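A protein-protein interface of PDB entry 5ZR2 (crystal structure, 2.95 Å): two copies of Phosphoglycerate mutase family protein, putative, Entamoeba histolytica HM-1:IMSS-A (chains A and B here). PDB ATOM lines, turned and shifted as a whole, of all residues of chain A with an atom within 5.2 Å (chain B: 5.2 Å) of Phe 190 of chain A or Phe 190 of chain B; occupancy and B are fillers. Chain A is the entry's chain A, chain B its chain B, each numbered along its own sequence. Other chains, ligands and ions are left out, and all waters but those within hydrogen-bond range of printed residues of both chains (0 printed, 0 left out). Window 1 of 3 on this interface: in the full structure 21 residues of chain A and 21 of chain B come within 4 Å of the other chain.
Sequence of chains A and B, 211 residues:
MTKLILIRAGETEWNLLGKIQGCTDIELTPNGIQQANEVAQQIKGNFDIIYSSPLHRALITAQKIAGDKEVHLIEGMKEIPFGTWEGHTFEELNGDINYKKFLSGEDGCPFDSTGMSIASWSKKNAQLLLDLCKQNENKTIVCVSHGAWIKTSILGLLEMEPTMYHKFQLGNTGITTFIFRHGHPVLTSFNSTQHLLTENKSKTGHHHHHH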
ATOM      1  N   ILE A 154     -27.512  -7.362   2.243  1.00  0.00           N
ATOM      2  CA  ILE A 154     -27.203  -8.566   1.463  1.00  0.00           C
ATOM      3  C   ILE A 154     -26.468  -9.575   2.351  1.00  0.00           C
ATOM      4  O   ILE A 154     -26.886 -10.733   2.459  1.00  0.00           O
ATOM      5  CB  ILE A 154     -26.371  -8.256   0.188  1.00  0.00           C
ATOM      6  CG1 ILE A 154     -27.165  -7.368  -0.785  1.00  0.00           C
ATOM      7  CG2 ILE A 154     -25.997  -9.542  -0.545  1.00  0.00           C
ATOM      8  CD1 ILE A 154     -26.323  -6.664  -1.837  1.00  0.00           C
ATOM      9  N   PHE A 168     -18.308  -6.858  -2.918  1.00  0.00           N
ATOM     10  CA  PHE A 168     -19.489  -6.437  -3.677  1.00  0.00           C
ATOM     11  C   PHE A 168     -19.347  -4.968  -4.009  1.00  0.00           C
ATOM     12  O   PHE A 168     -19.082  -4.170  -3.121  1.00  0.00           O
ATOM     13  CB  PHE A 168     -20.762  -6.602  -2.850  1.00  0.00           C
ATOM     14  CG  PHE A 168     -21.183  -8.029  -2.642  1.00  0.00           C
ATOM     15  CD1 PHE A 168     -20.576  -8.805  -1.669  1.00  0.00           C
ATOM     16  CD2 PHE A 168     -22.208  -8.591  -3.398  1.00  0.00           C
ATOM     17  CE1 PHE A 168     -20.965 -10.118  -1.459  1.00  0.00           C
ATOM     18  CE2 PHE A 168     -22.602  -9.904  -3.196  1.00  0.00           C
ATOM     19  CZ  PHE A 168     -21.983 -10.668  -2.223  1.00  0.00           C
ATOM     20  N   GLN A 169     -19.526  -4.613  -5.278  1.00  0.00           N
ATOM     21  CA  GLN A 169     -19.600  -3.208  -5.685  1.00  0.00           C
ATOM     22  C   GLN A 169     -20.969  -2.938  -6.284  1.00  0.00           C
ATOM     23  O   GLN A 169     -21.409  -3.650  -7.183  1.00  0.00           O
ATOM     24  CB  GLN A 169     -18.511  -2.863  -6.688  1.00  0.00           C
ATOM     25  CG  GLN A 169     -18.374  -1.371  -6.939  1.00  0.00           C
ATOM     26  CD  GLN A 169     -17.199  -1.046  -7.835  1.00  0.00           C
ATOM     27  OE1 GLN A 169     -16.228  -0.428  -7.403  1.00  0.00           O
ATOM     28  NE2 GLN A 169     -17.276  -1.471  -9.094  1.00  0.00           N
ATOM     29  N   LEU A 170     -21.622  -1.895  -5.783  1.00  0.00           N
ATOM     30  CA  LEU A 170     -23.018  -1.612  -6.083  1.00  0.00           C
ATOM     31  C   LEU A 170     -23.151  -0.212  -6.674  1.00  0.00           C
ATOM     32  O   LEU A 170     -22.742   0.763  -6.058  1.00  0.00           O
ATOM     33  CB  LEU A 170     -23.834  -1.738  -4.799  1.00  0.00           C
ATOM     34  CG  LEU A 170     -25.336  -1.458  -4.834  1.00  0.00           C
ATOM     35  CD1 LEU A 170     -26.057  -2.255  -5.910  1.00  0.00           C
ATOM     36  CD2 LEU A 170     -25.925  -1.759  -3.463  1.00  0.00           C
ATOM     37  N   ILE A 175     -29.948  -2.635  -9.374  1.00  0.00           N
ATOM     38  CA  ILE A 175     -31.030  -3.505  -8.902  1.00  0.00           C
ATOM     39  C   ILE A 175     -30.464  -4.796  -8.315  1.00  0.00           C
ATOM     40  O   ILE A 175     -29.641  -5.471  -8.937  1.00  0.00           O
ATOM     41  CB  ILE A 175     -32.063  -3.810 -10.007  1.00  0.00           C
ATOM     42  CG1 ILE A 175     -32.595  -2.487 -10.562  1.00  0.00           C
ATOM     43  CG2 ILE A 175     -33.210  -4.647  -9.451  1.00  0.00           C
ATOM     44  CD1 ILE A 175     -33.680  -2.613 -11.604  1.00  0.00           C
ATOM     45  N   THR A 176     -30.920  -5.108  -7.108  1.00  0.00           N
ATOM     46  CA  THR A 176     -30.539  -6.309  -6.381  1.00  0.00           C
ATOM     47  C   THR A 176     -31.846  -6.922  -5.911  1.00  0.00           C
ATOM     48  O   THR A 176     -32.681  -6.228  -5.334  1.00  0.00           O
ATOM     49  CB  THR A 176     -29.644  -5.963  -5.175  1.00  0.00           C
ATOM     50  OG1 THR A 176     -28.528  -5.170  -5.612  1.00  0.00           O
ATOM     51  CG2 THR A 176     -29.145  -7.233  -4.468  1.00  0.00           C
ATOM     52  N   THR A 177     -32.020  -8.213  -6.168  1.00  0.00           N
ATOM     53  CA  THR A 177     -33.295  -8.889  -5.941  1.00  0.00           C
ATOM     54  C   THR A 177     -33.119 -10.179  -5.160  1.00  0.00           C
ATOM     55  O   THR A 177     -32.139 -10.891  -5.348  1.00  0.00           O
ATOM     56  CB  THR A 177     -34.004  -9.199  -7.272  1.00  0.00           C
ATOM     57  OG1 THR A 177     -33.130  -9.943  -8.125  1.00  0.00           O
ATOM     58  CG2 THR A 177     -34.384  -7.915  -7.970  1.00  0.00           C
ATOM     59  N   LEU A 187     -30.466 -14.938  -3.414  1.00  0.00           N
ATOM     60  CA  LEU A 187     -30.102 -13.853  -4.314  1.00  0.00           C
ATOM     61  C   LEU A 187     -30.398 -14.283  -5.750  1.00  0.00           C
ATOM     62  O   LEU A 187     -29.843 -15.275  -6.225  1.00  0.00           O
ATOM     63  CB  LEU A 187     -28.615 -13.507  -4.154  1.00  0.00           C
ATOM     64  CG  LEU A 187     -28.064 -12.251  -4.842  1.00  0.00           C
ATOM     65  CD1 LEU A 187     -28.661 -10.991  -4.241  1.00  0.00           C
ATOM     66  CD2 LEU A 187     -26.548 -12.197  -4.739  1.00  0.00           C
ATOM     67  N   THR A 188     -31.297 -13.550  -6.412  1.00  0.00           N
ATOM     68  CA  THR A 188     -31.628 -13.768  -7.829  1.00  0.00           C
ATOM     69  C   THR A 188     -30.959 -12.776  -8.787  1.00  0.00           C
ATOM     70  O   THR A 188     -30.814 -13.075  -9.969  1.00  0.00           O
ATOM     71  CB  THR A 188     -33.145 -13.743  -8.065  1.00  0.00           C
ATOM     72  OG1 THR A 188     -33.689 -12.497  -7.618  1.00  0.00           O
ATOM     73  CG2 THR A 188     -33.799 -14.879  -7.314  1.00  0.00           C
ATOM     74  N   SER A 189     -30.577 -11.600  -8.293  1.00  0.00           N
ATOM     75  CA  SER A 189     -29.739 -10.667  -9.056  1.00  0.00           C
ATOM     76  C   SER A 189     -28.994  -9.756  -8.098  1.00  0.00           C
ATOM     77  O   SER A 189     -29.410  -9.590  -6.952  1.00  0.00           O
ATOM     78  CB  SER A 189     -30.565  -9.829 -10.041  1.00  0.00           C
ATOM     79  OG  SER A 189     -31.180  -8.719  -9.413  1.00  0.00           O
ATOM     80  N   PHE A 190     -27.890  -9.181  -8.569  1.00  0.00           N
ATOM     81  CA  PHE A 190     -27.158  -8.165  -7.815  1.00  0.00           C
ATOM     82  C   PHE A 190     -26.586  -7.113  -8.759  1.00  0.00           C
ATOM     83  O   PHE A 190     -25.993  -7.444  -9.782  1.00  0.00           O
ATOM     84  CB  PHE A 190     -26.036  -8.770  -6.959  1.00  0.00           C
ATOM     85  CG  PHE A 190     -25.063  -7.742  -6.439  1.00  0.00           C
ATOM     86  CD1 PHE A 190     -25.438  -6.863  -5.435  1.00  0.00           C
ATOM     87  CD2 PHE A 190     -23.795  -7.614  -6.991  1.00  0.00           C
ATOM     88  CE1 PHE A 190     -24.563  -5.897  -4.970  1.00  0.00           C
ATOM     89  CE2 PHE A 190     -22.916  -6.645  -6.530  1.00  0.00           C
ATOM     90  CZ  PHE A 190     -23.303  -5.788  -5.519  1.00  0.00           C
ATOM     91  N   ASN A 191     -26.765  -5.850  -8.375  1.00  0.00           N
ATOM     92  CA  ASN A 191     -26.277  -4.680  -9.109  1.00  0.00           C
ATOM     93  C   ASN A 191     -26.500  -4.712 -10.617  1.00  0.00           C
ATOM     94  O   ASN A 191     -25.618  -4.357 -11.406  1.00  0.00           O
ATOM     95  CB  ASN A 191     -24.800  -4.423  -8.803  1.00  0.00           C
ATOM     96  CG  ASN A 191     -24.333  -3.062  -9.307  1.00  0.00           C
ATOM     97  OD1 ASN A 191     -25.111  -2.105  -9.363  1.00  0.00           O
ATOM     98  ND2 ASN A 191     -23.064  -2.964  -9.669  1.00  0.00           N
ATOM     99  N   SER A 192     -27.691  -5.140 -11.003  1.00  0.00           N
ATOM    100  CA  SER A 192     -28.102  -5.097 -12.390  1.00  0.00           C
ATOM    101  C   SER A 192     -28.287  -3.625 -12.797  1.00  0.00           C
ATOM    102  O   SER A 192     -29.086  -2.906 -12.198  1.00  0.00           O
ATOM    103  CB  SER A 192     -29.383  -5.903 -12.577  1.00  0.00           C
ATOM    104  OG  SER A 192     -29.997  -5.592 -13.806  1.00  0.00           O
ATOM    105  N   ILE B 154     -17.906 -18.248  -8.632  1.00  0.00           N
ATOM    106  CA  ILE B 154     -18.217 -17.085  -7.790  1.00  0.00           C
ATOM    107  C   ILE B 154     -17.736 -17.332  -6.364  1.00  0.00           C
ATOM    108  O   ILE B 154     -17.001 -16.519  -5.805  1.00  0.00           O
ATOM    109  CB  ILE B 154     -19.729 -16.749  -7.782  1.00  0.00           C
ATOM    110  CG1 ILE B 154     -20.197 -16.307  -9.170  1.00  0.00           C
ATOM    111  CG2 ILE B 154     -20.036 -15.623  -6.801  1.00  0.00           C
ATOM    112  CD1 ILE B 154     -21.692 -16.425  -9.380  1.00  0.00           C
ATOM    113  N   PHE B 168     -27.448 -18.546  -4.169  1.00  0.00           N
ATOM    114  CA  PHE B 168     -27.369 -17.874  -5.470  1.00  0.00           C
ATOM    115  C   PHE B 168     -28.230 -18.613  -6.478  1.00  0.00           C
ATOM    116  O   PHE B 168     -28.145 -19.836  -6.566  1.00  0.00           O
ATOM    117  CB  PHE B 168     -25.935 -17.859  -5.989  1.00  0.00           C
ATOM    118  CG  PHE B 168     -25.032 -16.919  -5.253  1.00  0.00           C
ATOM    119  CD1 PHE B 168     -24.423 -17.314  -4.075  1.00  0.00           C
ATOM    120  CD2 PHE B 168     -24.772 -15.646  -5.745  1.00  0.00           C
ATOM    121  CE1 PHE B 168     -23.578 -16.460  -3.386  1.00  0.00           C
ATOM    122  CE2 PHE B 168     -23.929 -14.783  -5.065  1.00  0.00           C
ATOM    123  CZ  PHE B 168     -23.330 -15.189  -3.881  1.00  0.00           C
ATOM    124  N   GLN B 169     -29.041 -17.871  -7.234  1.00  0.00           N
ATOM    125  CA  GLN B 169     -29.835 -18.439  -8.327  1.00  0.00           C
ATOM    126  C   GLN B 169     -29.539 -17.721  -9.634  1.00  0.00           C
ATOM    127  O   GLN B 169     -29.759 -16.523  -9.755  1.00  0.00           O
ATOM    128  CB  GLN B 169     -31.330 -18.372  -8.033  1.00  0.00           C
ATOM    129  CG  GLN B 169     -32.144 -19.306  -8.918  1.00  0.00           C
ATOM    130  CD  GLN B 169     -33.630 -19.045  -8.835  1.00  0.00           C
ATOM    131  OE1 GLN B 169     -34.378 -19.823  -8.239  1.00  0.00           O
ATOM    132  NE2 GLN B 169     -34.069 -17.944  -9.434  1.00  0.00           N
ATOM    133  N   LEU B 170     -29.076 -18.487 -10.615  1.00  0.00           N
ATOM    134  CA  LEU B 170     -28.545 -17.964 -11.864  1.00  0.00           C
ATOM    135  C   LEU B 170     -29.410 -18.447 -13.019  1.00  0.00           C
ATOM    136  O   LEU B 170     -29.769 -19.619 -13.087  1.00  0.00           O
ATOM    137  CB  LEU B 170     -27.097 -18.432 -12.024  1.00  0.00           C
ATOM    138  CG  LEU B 170     -26.271 -18.018 -13.243  1.00  0.00           C
ATOM    139  CD1 LEU B 170     -26.267 -16.512 -13.471  1.00  0.00           C
ATOM    140  CD2 LEU B 170     -24.846 -18.536 -13.065  1.00  0.00           C
ATOM    141  N   ILE B 175     -25.947 -12.591 -16.764  1.00  0.00           N
ATOM    142  CA  ILE B 175     -24.624 -11.970 -16.762  1.00  0.00           C
ATOM    143  C   ILE B 175     -24.148 -11.792 -15.320  1.00  0.00           C
ATOM    144  O   ILE B 175     -24.916 -11.410 -14.435  1.00  0.00           O
ATOM    145  CB  ILE B 175     -24.598 -10.625 -17.532  1.00  0.00           C
ATOM    146  CG1 ILE B 175     -25.040 -10.859 -18.983  1.00  0.00           C
ATOM    147  CG2 ILE B 175     -23.197  -9.999 -17.486  1.00  0.00           C
ATOM    148  CD1 ILE B 175     -25.003  -9.638 -19.874  1.00  0.00           C
ATOM    149  N   THR B 176     -22.865 -12.070 -15.120  1.00  0.00           N
ATOM    150  CA  THR B 176     -22.203 -11.999 -13.822  1.00  0.00           C
ATOM    151  C   THR B 176     -20.816 -11.440 -14.107  1.00  0.00           C
ATOM    152  O   THR B 176     -20.106 -11.963 -14.961  1.00  0.00           O
ATOM    153  CB  THR B 176     -22.095 -13.392 -13.173  1.00  0.00           C
ATOM    154  OG1 THR B 176     -23.402 -13.968 -13.044  1.00  0.00           O
ATOM    155  CG2 THR B 176     -21.442 -13.319 -11.804  1.00  0.00           C
ATOM    156  N   THR B 177     -20.444 -10.377 -13.401  1.00  0.00           N
ATOM    157  CA  THR B 177     -19.224  -9.626 -13.709  1.00  0.00           C
ATOM    158  C   THR B 177     -18.341  -9.422 -12.480  1.00  0.00           C
ATOM    159  O   THR B 177     -18.835  -9.269 -11.362  1.00  0.00           O
ATOM    160  CB  THR B 177     -19.542  -8.252 -14.349  1.00  0.00           C
ATOM    161  OG1 THR B 177     -20.448  -7.520 -13.521  1.00  0.00           O
ATOM    162  CG2 THR B 177     -20.171  -8.429 -15.703  1.00  0.00           C
ATOM    163  N   LEU B 187     -17.108  -8.574  -7.027  1.00  0.00           N
ATOM    164  CA  LEU B 187     -18.343  -8.780  -7.787  1.00  0.00           C
ATOM    165  C   LEU B 187     -19.011  -7.437  -8.100  1.00  0.00           C
ATOM    166  O   LEU B 187     -19.349  -6.687  -7.188  1.00  0.00           O
ATOM    167  CB  LEU B 187     -19.309  -9.671  -6.990  1.00  0.00           C
ATOM    168  CG  LEU B 187     -20.616 -10.129  -7.661  1.00  0.00           C
ATOM    169  CD1 LEU B 187     -20.346 -11.175  -8.727  1.00  0.00           C
ATOM    170  CD2 LEU B 187     -21.594 -10.683  -6.634  1.00  0.00           C
ATOM    171  N   THR B 188     -19.177  -7.141  -9.389  1.00  0.00           N
ATOM    172  CA  THR B 188     -19.857  -5.917  -9.839  1.00  0.00           C
ATOM    173  C   THR B 188     -21.280  -6.142 -10.339  1.00  0.00           C
ATOM    174  O   THR B 188     -22.065  -5.200 -10.391  1.00  0.00           O
ATOM    175  CB  THR B 188     -19.072  -5.210 -10.947  1.00  0.00           C
ATOM    176  OG1 THR B 188     -18.880  -6.106 -12.045  1.00  0.00           O
ATOM    177  CG2 THR B 188     -17.737  -4.749 -10.419  1.00  0.00           C
ATOM    178  N   SER B 189     -21.598  -7.366 -10.747  1.00  0.00           N
ATOM    179  CA  SER B 189     -22.980  -7.753 -11.025  1.00  0.00           C
ATOM    180  C   SER B 189     -23.117  -9.263 -10.894  1.00  0.00           C
ATOM    181  O   SER B 189     -22.135  -9.992 -11.067  1.00  0.00           O
ATOM    182  CB  SER B 189     -23.427  -7.284 -12.419  1.00  0.00           C
ATOM    183  OG  SER B 189     -22.955  -8.133 -13.453  1.00  0.00           O
ATOM    184  N   PHE B 190     -24.325  -9.717 -10.565  1.00  0.00           N
ATOM    185  CA  PHE B 190     -24.652 -11.141 -10.588  1.00  0.00           C
ATOM    186  C   PHE B 190     -26.017 -11.371 -11.222  1.00  0.00           C
ATOM    187  O   PHE B 190     -26.977 -10.684 -10.889  1.00  0.00           O
ATOM    188  CB  PHE B 190     -24.628 -11.754  -9.188  1.00  0.00           C
ATOM    189  CG  PHE B 190     -25.258 -13.116  -9.127  1.00  0.00           C
ATOM    190  CD1 PHE B 190     -24.639 -14.201  -9.732  1.00  0.00           C
ATOM    191  CD2 PHE B 190     -26.491 -13.306  -8.507  1.00  0.00           C
ATOM    192  CE1 PHE B 190     -25.219 -15.458  -9.698  1.00  0.00           C
ATOM    193  CE2 PHE B 190     -27.079 -14.563  -8.471  1.00  0.00           C
ATOM    194  CZ  PHE B 190     -26.441 -15.640  -9.067  1.00  0.00           C
ATOM    195  N   ASN B 191     -26.078 -12.355 -12.118  1.00  0.00           N
ATOM    196  CA  ASN B 191     -27.308 -12.783 -12.795  1.00  0.00           C
ATOM    197  C   ASN B 191     -28.169 -11.631 -13.334  1.00  0.00           C
ATOM    198  O   ASN B 191     -29.388 -11.594 -13.138  1.00  0.00           O
ATOM    199  CB  ASN B 191     -28.130 -13.707 -11.879  1.00  0.00           C
ATOM    200  CG  ASN B 191     -29.301 -14.365 -12.599  1.00  0.00           C
ATOM    201  OD1 ASN B 191     -29.263 -14.586 -13.810  1.00  0.00           O
ATOM    202  ND2 ASN B 191     -30.346 -14.688 -11.856  1.00  0.00           N
ATOM    203  N   SER B 192     -27.514 -10.690 -14.002  1.00  0.00           N
ATOM    204  CA  SER B 192     -28.207  -9.599 -14.674  1.00  0.00           C
ATOM    205  C   SER B 192     -28.893 -10.151 -15.921  1.00  0.00           C
ATOM    206  O   SER B 192     -28.228 -10.692 -16.800  1.00  0.00           O
ATOM    207  CB  SER B 192     -27.224  -8.489 -15.044  1.00  0.00           C
ATOM    208  OG  SER B 192     -27.861  -7.468 -15.796  1.00  0.00           O
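Among the printed residues, merely in contact across the chains: Phe 190 of chain A with Ser 189 of chain B (3.3 Å), Ser 189 of chain A with Phe 190 of chain B (3.3 Å), Phe 168 of chain A with Leu 187 of chain B (3.5 Å), Gln 169 of chain A with Thr 188 of chain B (3.6 Å), Thr 188 of chain A with Gln 169 of chain B (3.6 Å), Phe 190 of chain A with Leu 187 of chain B (3.6 Å), Leu 187 of chain A with Phe 190 of chain B (3.6 Å), Leu 187 of chain A with Phe 168 of chain B (3.7 Å), Ser 189 of chain A with Asn 191 of chain B (3.8 Å) and Asn 191 of chain A with Ser 189 of chain B (3.8 Å).
The backbone NH (N) of Gln 169 of chain A sits at hydrogen-bond distance from the backbone carbonyl oxygen (O) of Leu 187 of chain B, 2.8 Å away.
The backbone carbonyl oxygen (O) of Leu 187 of chain A is in hydrogen-bond range of the backbone NH (N) of Gln 169 of chain B.
O of Thr 188 of chain A sits at hydrogen-bond distance from ND2 of Asn 191 of chain B (2.5 Å).
O of Phe 190 of chain B sits at hydrogen-bond distance from N of Phe 190 of chain A (2.9 Å).
The backbone carbonyl oxygen (O) of Thr 188 of chain B is in hydrogen-bond range of the side-chain amide nitrogen (ND2) of Asn 191 of chain A.
The side-chain hydroxyl (OG) of Ser 192 of chain A sits at hydrogen-bond distance from the side-chain hydroxyl (OG) of Ser 192 of chain B (3.5 Å).
Leu 170 of chain A touches none of the printed residues of chain B.
Printed residues of chain B within 4 Å of Ser 189 of chain A: Phe 190 (3.3 Å) and Asn 191 (3.8 Å).
Phe 190 of chain A touches just these residues of chain B: Leu 187 (3.6 Å), Ser 189 (3.3 Å) and Phe 190 (2.9 Å).
Printed residues of chain B within 4 Å of Ser 192 of chain A: Ser 192.
Of the printed residues of chain A, Leu 187 of chain B touches Phe 168, Gln 169 and Phe 190.
Of the printed residues of chain A, Ser 189 of chain B touches Phe 190 (3.3 Å) and Asn 191 (3.8 Å).
Of chain A, only Leu 187, Ser 189 and Phe 190 come within 4 Å of Phe 190 of chain B.
The nearest residue of chain A that does not touch Phe 190 of chain B is Thr 188 of chain A (4.3 Å).
The nearest printed residue of chain A that does not touch Thr 188 of chain B is Phe 190 of chain A (4.2 Å).
Phe 168 of chain A touches Leu 187 of chain B, and with the chains exchanged Leu 187 of chain A touches Phe 168 of chain B.
Gln 169 of chain A touches Leu 187 of chain B, and with the chains exchanged Leu 187 of chain A touches Gln 169 of chain B.
Ser 189 of chain A touches Asn 191 of chain B, and with the chains exchanged Asn 191 of chain A touches Ser 189 of chain B.
Phe 190 of chain B touches its own counterpart, Phe 190 of chain A.
Of the 16 pairs that touch across the chains among the printed residues, 16 have their exchanged pair printed and touching as well.
ND2 of Asn 191 of chain A sits at hydrogen-bond distance from O of Gln 169 of chain A.
The backbone carbonyl oxygen (O) of Ile 175 of chain A is in hydrogen-bond range of the backbone NH (N) of Ser 192 of chain A (2.9 Å).
The side-chain hydroxyl (OG1) of Thr 177 of chain A lies within hydrogen-bond range of the side-chain hydroxyl (OG1) of Thr 188 of chain A (2.7 Å).
OG1 of Thr 177 of chain A sits at hydrogen-bond distance from OG of Ser 189 of chain A, at 2.6 Å.
The backbone carbonyl oxygen (O) of Ile 175 of chain B lies within hydrogen-bond range of the backbone NH (N) of Asn 191 of chain B (2.8 Å).
The side-chain hydroxyl (OG1) of Thr 177 of chain B is in hydrogen-bond range of the side-chain hydroxyl (OG1) of Thr 188 of chain B, 2.6 Å away.
Printed residues of chain B that touch a printed residue of chain A: Phe 168, Gln 169, Leu 187, Thr 188, Ser 189, Phe 190, Asn 191 and Ser 192.
Hydrophobic or aromatic side chains of chain B within 4 Å of the printed part of chain A: Phe 168, Leu 187 and Phe 190.
Hydrophobic or aromatic side chains of chain A that line the printed part of chain B: Phe 168, Leu 187 and Phe 190.
Among the printed residues, 16 pairs touch across the chains.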
